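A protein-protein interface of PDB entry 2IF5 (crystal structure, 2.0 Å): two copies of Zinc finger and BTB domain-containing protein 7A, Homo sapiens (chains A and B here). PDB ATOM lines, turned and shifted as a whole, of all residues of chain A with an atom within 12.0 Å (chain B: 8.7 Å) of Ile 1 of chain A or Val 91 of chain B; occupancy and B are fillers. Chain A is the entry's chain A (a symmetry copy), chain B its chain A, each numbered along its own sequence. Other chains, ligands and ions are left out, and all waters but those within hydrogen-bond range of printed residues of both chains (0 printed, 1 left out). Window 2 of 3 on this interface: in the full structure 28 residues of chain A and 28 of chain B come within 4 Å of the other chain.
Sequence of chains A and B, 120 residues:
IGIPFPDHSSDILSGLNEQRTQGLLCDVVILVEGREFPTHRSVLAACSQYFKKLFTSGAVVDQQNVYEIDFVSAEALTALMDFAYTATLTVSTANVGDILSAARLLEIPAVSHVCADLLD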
ATOM      1  N   ILE A   1      24.764  23.449  -8.506  1.00  0.00           N
ATOM      2  CA  ILE A   1      25.290  24.677  -9.093  1.00  0.00           C
ATOM      3  C   ILE A   1      25.737  25.514  -7.910  1.00  0.00           C
ATOM      4  O   ILE A   1      25.080  25.546  -6.856  1.00  0.00           O
ATOM      5  CB  ILE A   1      24.268  25.316 -10.092  1.00  0.00           C
ATOM      6  CG1 ILE A   1      24.858  26.492 -10.883  1.00  0.00           C
ATOM      7  CG2 ILE A   1      22.965  25.634  -9.449  1.00  0.00           C
ATOM      8  CD1 ILE A   1      25.437  26.106 -12.241  1.00  0.00           C
ATOM      9  N   GLY A   2      26.902  26.134  -8.066  1.00  0.00           N
ATOM     10  CA  GLY A   2      27.677  26.615  -6.925  1.00  0.00           C
ATOM     11  C   GLY A   2      26.967  27.620  -6.044  1.00  0.00           C
ATOM     12  O   GLY A   2      26.756  28.755  -6.501  1.00  0.00           O
ATOM     13  N   ILE A   3      26.537  27.199  -4.823  1.00  0.00           N
ATOM     14  CA  ILE A   3      26.137  28.161  -3.782  1.00  0.00           C
ATOM     15  C   ILE A   3      27.419  28.815  -3.279  1.00  0.00           C
ATOM     16  O   ILE A   3      28.292  28.111  -2.810  1.00  0.00           O
ATOM     17  CB  ILE A   3      25.413  27.525  -2.555  1.00  0.00           C
ATOM     18  CG1 ILE A   3      24.091  26.816  -2.920  1.00  0.00           C
ATOM     19  CG2 ILE A   3      25.118  28.597  -1.467  1.00  0.00           C
ATOM     20  CD1 ILE A   3      23.510  26.065  -1.714  1.00  0.00           C
ATOM     21  N   PRO A   4      27.537  30.153  -3.396  1.00  0.00           N
ATOM     22  CA  PRO A   4      28.742  30.826  -2.964  1.00  0.00           C
ATOM     23  C   PRO A   4      28.671  31.164  -1.475  1.00  0.00           C
ATOM     24  O   PRO A   4      27.617  31.621  -0.995  1.00  0.00           O
ATOM     25  CB  PRO A   4      28.722  32.126  -3.793  1.00  0.00           C
ATOM     26  CG  PRO A   4      27.281  32.351  -4.154  1.00  0.00           C
ATOM     27  CD  PRO A   4      26.533  31.094  -3.948  1.00  0.00           C
ATOM     28  N   PHE A   5      29.787  30.969  -0.784  1.00  0.00           N
ATOM     29  CA  PHE A   5      29.957  31.312   0.652  1.00  0.00           C
ATOM     30  C   PHE A   5      31.038  32.396   0.791  1.00  0.00           C
ATOM     31  O   PHE A   5      32.227  32.105   1.021  1.00  0.00           O
ATOM     32  CB  PHE A   5      30.320  30.083   1.497  1.00  0.00           C
ATOM     33  CG  PHE A   5      29.210  29.070   1.592  1.00  0.00           C
ATOM     34  CD1 PHE A   5      28.877  28.270   0.501  1.00  0.00           C
ATOM     35  CD2 PHE A   5      28.474  28.941   2.772  1.00  0.00           C
ATOM     36  CE1 PHE A   5      27.852  27.312   0.596  1.00  0.00           C
ATOM     37  CE2 PHE A   5      27.442  28.003   2.870  1.00  0.00           C
ATOM     38  CZ  PHE A   5      27.122  27.192   1.776  1.00  0.00           C
ATOM     39  N   ALA B  79      31.414  16.623  -2.655  1.00  0.00           N
ATOM     40  CA  ALA B  79      30.849  17.970  -2.753  1.00  0.00           C
ATOM     41  C   ALA B  79      31.231  18.823  -1.553  1.00  0.00           C
ATOM     42  O   ALA B  79      31.529  20.014  -1.691  1.00  0.00           O
ATOM     43  CB  ALA B  79      29.330  17.905  -2.924  1.00  0.00           C
ATOM     44  N   LEU B  80      31.233  18.227  -0.369  1.00  0.00           N
ATOM     45  CA  LEU B  80      31.581  18.979   0.844  1.00  0.00           C
ATOM     46  C   LEU B  80      33.076  19.273   0.970  1.00  0.00           C
ATOM     47  O   LEU B  80      33.494  20.320   1.529  1.00  0.00           O
ATOM     48  CB  LEU B  80      31.065  18.211   2.075  1.00  0.00           C
ATOM     49  CG  LEU B  80      29.560  18.273   2.268  1.00  0.00           C
ATOM     50  CD1 LEU B  80      29.167  17.207   3.275  1.00  0.00           C
ATOM     51  CD2 LEU B  80      29.148  19.665   2.762  1.00  0.00           C
ATOM     52  N   THR B  88      32.550  27.295  -2.418  1.00  0.00           N
ATOM     53  CA  THR B  88      31.386  27.080  -3.280  1.00  0.00           C
ATOM     54  C   THR B  88      30.897  25.662  -3.103  1.00  0.00           C
ATOM     55  O   THR B  88      31.687  24.712  -3.204  1.00  0.00           O
ATOM     56  CB  THR B  88      31.762  27.250  -4.791  1.00  0.00           C
ATOM     57  OG1 THR B  88      32.306  28.553  -5.013  1.00  0.00           O
ATOM     58  CG2 THR B  88      30.549  27.125  -5.657  1.00  0.00           C
ATOM     59  N   LEU B  89      29.591  25.518  -2.872  1.00  0.00           N
ATOM     60  CA  LEU B  89      28.989  24.218  -2.758  1.00  0.00           C
ATOM     61  C   LEU B  89      28.202  23.975  -4.021  1.00  0.00           C
ATOM     62  O   LEU B  89      27.234  24.681  -4.308  1.00  0.00           O
ATOM     63  CB  LEU B  89      28.047  24.176  -1.549  1.00  0.00           C
ATOM     64  CG  LEU B  89      27.250  22.876  -1.378  1.00  0.00           C
ATOM     65  CD1 LEU B  89      28.283  21.783  -1.039  1.00  0.00           C
ATOM     66  CD2 LEU B  89      26.311  23.077  -0.192  1.00  0.00           C
ATOM     67  N   THR B  90      28.614  22.975  -4.779  1.00  0.00           N
ATOM     68  CA  THR B  90      27.904  22.632  -5.976  1.00  0.00           C
ATOM     69  C   THR B  90      26.864  21.614  -5.601  1.00  0.00           C
ATOM     70  O   THR B  90      27.180  20.570  -5.056  1.00  0.00           O
ATOM     71  CB  THR B  90      28.882  22.068  -7.035  1.00  0.00           C
ATOM     72  OG1 THR B  90      29.556  20.928  -6.474  1.00  0.00           O
ATOM     73  CG2 THR B  90      29.880  23.061  -7.306  1.00  0.00           C
ATOM     74  N   VAL B  91      25.603  21.930  -5.890  1.00  0.00           N
ATOM     75  CA  VAL B  91      24.511  21.079  -5.529  1.00  0.00           C
ATOM     76  C   VAL B  91      23.392  21.343  -6.539  1.00  0.00           C
ATOM     77  O   VAL B  91      23.185  22.466  -6.997  1.00  0.00           O
ATOM     78  CB  VAL B  91      24.050  21.285  -4.032  1.00  0.00           C
ATOM     79  CG1 VAL B  91      23.575  22.718  -3.755  1.00  0.00           C
ATOM     80  CG2 VAL B  91      22.953  20.269  -3.655  1.00  0.00           C
ATOM     81  N   SER B  92      22.646  20.316  -6.858  1.00  0.00           N
ATOM     82  CA  SER B  92      21.443  20.536  -7.664  1.00  0.00           C
ATOM     83  C   SER B  92      20.219  20.692  -6.760  1.00  0.00           C
ATOM     84  O   SER B  92      20.239  20.352  -5.593  1.00  0.00           O
ATOM     85  CB  SER B  92      21.251  19.351  -8.568  1.00  0.00           C
ATOM     86  OG  SER B  92      20.817  18.290  -7.740  1.00  0.00           O
ATOM     87  N   THR B  93      19.125  21.158  -7.341  1.00  0.00           N
ATOM     88  CA  THR B  93      17.920  21.416  -6.588  1.00  0.00           C
ATOM     89  C   THR B  93      17.424  20.138  -5.898  1.00  0.00           C
ATOM     90  O   THR B  93      16.952  20.188  -4.759  1.00  0.00           O
ATOM     91  CB  THR B  93      16.856  22.023  -7.513  1.00  0.00           C
ATOM     92  OG1 THR B  93      15.933  22.788  -6.733  1.00  0.00           O
ATOM     93  CG2 THR B  93      16.144  20.951  -8.313  1.00  0.00           C
ATOM     94  N   ALA B  94      17.576  18.990  -6.576  1.00  0.00           N
ATOM     95  CA  ALA B  94      17.155  17.706  -5.993  1.00  0.00           C
ATOM     96  C   ALA B  94      18.010  17.166  -4.881  1.00  0.00           C
ATOM     97  O   ALA B  94      17.516  16.371  -4.091  1.00  0.00           O
ATOM     98  CB  ALA B  94      16.975  16.652  -7.036  1.00  0.00           C
ATOM     99  N   ASN B  95      19.262  17.615  -4.789  1.00  0.00           N
ATOM    100  CA  ASN B  95      20.211  17.071  -3.832  1.00  0.00           C
ATOM    101  C   ASN B  95      20.396  17.900  -2.587  1.00  0.00           C
ATOM    102  O   ASN B  95      21.093  17.471  -1.696  1.00  0.00           O
ATOM    103  CB  ASN B  95      21.594  16.871  -4.495  1.00  0.00           C
ATOM    104  CG  ASN B  95      21.625  15.654  -5.402  1.00  0.00           C
ATOM    105  OD1 ASN B  95      20.688  14.840  -5.393  1.00  0.00           O
ATOM    106  ND2 ASN B  95      22.693  15.532  -6.217  1.00  0.00           N
ATOM    107  N   VAL B  96      19.791  19.087  -2.512  1.00  0.00           N
ATOM    108  CA  VAL B  96      19.959  19.923  -1.302  1.00  0.00           C
ATOM    109  C   VAL B  96      19.740  19.131  -0.004  1.00  0.00           C
ATOM    110  O   VAL B  96      20.581  19.177   0.911  1.00  0.00           O
ATOM    111  CB  VAL B  96      19.099  21.217  -1.346  1.00  0.00           C
ATOM    112  CG1 VAL B  96      19.145  21.951   0.013  1.00  0.00           C
ATOM    113  CG2 VAL B  96      19.627  22.129  -2.441  1.00  0.00           C
ATOM    114  N   GLY B  97      18.661  18.352   0.055  1.00  0.00           N
ATOM    115  CA  GLY B  97      18.363  17.562   1.277  1.00  0.00           C
ATOM    116  C   GLY B  97      19.411  16.500   1.589  1.00  0.00           C
ATOM    117  O   GLY B  97      19.730  16.235   2.752  1.00  0.00           O
ATOM    118  N   ASP B  98      19.966  15.891   0.548  1.00  0.00           N
ATOM    119  CA  ASP B  98      21.091  14.938   0.741  1.00  0.00           C
ATOM    120  C   ASP B  98      22.352  15.603   1.340  1.00  0.00           C
ATOM    121  O   ASP B  98      23.047  15.074   2.240  1.00  0.00           O
ATOM    122  CB  ASP B  98      21.417  14.366  -0.629  1.00  0.00           C
ATOM    123  CG  ASP B  98      20.218  13.660  -1.227  1.00  0.00           C
ATOM    124  OD1 ASP B  98      19.884  12.596  -0.694  1.00  0.00           O
ATOM    125  OD2 ASP B  98      19.562  14.214  -2.140  1.00  0.00           O
ATOM    126  N   ILE B  99      22.673  16.779   0.820  1.00  0.00           N
ATOM    127  CA  ILE B  99      23.850  17.471   1.335  1.00  0.00           C
ATOM    128  C   ILE B  99      23.603  17.935   2.784  1.00  0.00           C
ATOM    129  O   ILE B  99      24.516  17.870   3.633  1.00  0.00           O
ATOM    130  CB  ILE B  99      24.274  18.642   0.420  1.00  0.00           C
ATOM    131  CG1 ILE B  99      24.564  18.155  -1.017  1.00  0.00           C
ATOM    132  CG2 ILE B  99      25.513  19.423   1.043  1.00  0.00           C
ATOM    133  CD1 ILE B  99      25.757  17.168  -1.222  1.00  0.00           C
ATOM    134  N   LEU B 100      22.379  18.382   3.065  1.00  0.00           N
ATOM    135  CA  LEU B 100      21.986  18.794   4.415  1.00  0.00           C
ATOM    136  C   LEU B 100      22.230  17.630   5.361  1.00  0.00           C
ATOM    137  O   LEU B 100      22.844  17.820   6.382  1.00  0.00           O
ATOM    138  CB  LEU B 100      20.506  19.183   4.478  1.00  0.00           C
ATOM    139  CG  LEU B 100      19.968  19.502   5.870  1.00  0.00           C
ATOM    140  CD1 LEU B 100      20.858  20.531   6.603  1.00  0.00           C
ATOM    141  CD2 LEU B 100      18.509  19.960   5.772  1.00  0.00           C
ATOM    142  N   VAL B 111      27.132  25.074   5.966  1.00  0.00           N
ATOM    143  CA  VAL B 111      26.357  24.361   4.957  1.00  0.00           C
ATOM    144  C   VAL B 111      25.003  23.892   5.505  1.00  0.00           C
ATOM    145  O   VAL B 111      23.958  24.016   4.807  1.00  0.00           O
ATOM    146  CB  VAL B 111      27.170  23.177   4.364  1.00  0.00           C
ATOM    147  CG1 VAL B 111      26.259  22.290   3.482  1.00  0.00           C
ATOM    148  CG2 VAL B 111      28.364  23.723   3.551  1.00  0.00           C
ATOM    149  N   VAL B 114      22.372  26.830   5.808  1.00  0.00           N
ATOM    150  CA  VAL B 114      21.931  27.247   4.484  1.00  0.00           C
ATOM    151  C   VAL B 114      21.002  26.211   3.844  1.00  0.00           C
ATOM    152  O   VAL B 114      19.930  26.543   3.373  1.00  0.00           O
ATOM    153  CB  VAL B 114      23.143  27.533   3.590  1.00  0.00           C
ATOM    154  CG1 VAL B 114      22.715  27.673   2.129  1.00  0.00           C
ATOM    155  CG2 VAL B 114      23.802  28.822   4.097  1.00  0.00           C
ATOM    156  N   CYS B 115      21.410  24.951   3.820  1.00  0.00           N
ATOM    157  CA  CYS B 115      20.589  23.934   3.168  1.00  0.00           C
ATOM    158  C   CYS B 115      19.229  23.782   3.868  1.00  0.00           C
ATOM    159  O   CYS B 115      18.204  23.574   3.209  1.00  0.00           O
ATOM    160  CB  CYS B 115      21.357  22.617   3.058  1.00  0.00           C
ATOM    161  SG  CYS B 115      22.687  22.710   1.859  1.00  0.00           S
ATOM    162  N   LEU B 118      17.006  26.400   2.718  1.00  0.00           N
ATOM    163  CA  LEU B 118      16.578  26.210   1.317  1.00  0.00           C
ATOM    164  C   LEU B 118      15.463  25.207   1.225  1.00  0.00           C
ATOM    165  O   LEU B 118      14.715  25.211   0.272  1.00  0.00           O
ATOM    166  CB  LEU B 118      17.744  25.751   0.430  1.00  0.00           C
ATOM    167  CG  LEU B 118      18.850  26.797   0.194  1.00  0.00           C
ATOM    168  CD1 LEU B 118      19.962  26.156  -0.587  1.00  0.00           C
ATOM    169  CD2 LEU B 118      18.262  27.973  -0.611  1.00  0.00           C
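No position is printed for both chains.
N of Ile 1 of chain A sits close to O of Val 91 of chain B (2.4 Å). The backbone carbonyl oxygen of Ile 1 of chain A sits close to the backbone carbonyl oxygen of Leu 89 of chain B (3.4 Å). The backbone NH (N) of Ile 3 of chain A lies within hydrogen-bond range of the backbone carbonyl oxygen (O) of Leu 89 of chain B, 2.7 Å away.
Of the 19 printed residues of chain B, 5 touch a printed residue of chain A. Along chain B the printed residues that touch a printed residue of chain A span positions 88 to 118. Of the 5 printed residues of chain A, 4 touch a printed residue of chain B. Among the printed residues, 10 pairs touch across the chains.
Of chain B, only Leu 89 (3.4 Å) and Val 91 (2.4 Å) come within 4 Å of Ile 1 of chain A. Val 91 of chain B touches two residues of chain A. Of chain A, only Ile 1 (3.4 Å), Gly 2 (3.3 Å), Ile 3 (2.7 Å) and Phe 5 (3.8 Å) come within 4 Å of Leu 89 of chain B. No residue of chain A comes within 4 Å of Thr 90 of chain B. No residue of chain A comes within 4 Å of Ser 92 of chain B. Thr 93 of chain B touches none of the printed residues of chain A. No residue of chain A comes within 4 Å of Val 96 of chain B. No residue of chain A comes within 4 Å of Ile 99 of chain B. Of the printed residues of chain A, Leu 118 of chain B touches Ile 3 (3.7 Å). Of the printed residues of chain A, Val 114 of chain B touches Phe 5. Printed residues of chain B within 4 Å of Ile 3 of chain A: Thr 88 (3.3 Å), Leu 89 (2.7 Å), Val 91 (3.9 Å) and Leu 118 (3.7 Å). Of the printed residues of chain A, Thr 88 of chain B touches Gly 2 and Ile 3. Of the printed residues of chain B, Phe 5 of chain A touches Leu 89 (3.8 Å) and Val 114 (3.9 Å). Pro 4 of chain A touches none of the printed residues of chain B. Cys 115 of chain B touches none of the printed residues of chain A. The nearest residue of chain B that does not touch Ile 1 of chain A is Thr 90 of chain B (4.03 Å).
CG2 of Thr 88 of chain B touches CA of Gly 2 of chain A, at 3.2 Å. Leu 89 of chain B touches Gly 2 of chain A (O to CA, 3.3 Å). Ile 3 of chain A touches Thr 88 of chain B (O to CA, 3.3 Å). CG1 of Val 91 of chain B touches CD1 of Ile 3 of chain A, 3.9 Å away. CD1 of Leu 118 of chain B touches CD1 of Ile 3 of chain A (3.7 Å). Phe 5 of chain A touches Leu 89 of chain B (CE1 to CB, 3.8 Å). Phe 5 of chain A touches Val 114 of chain B.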
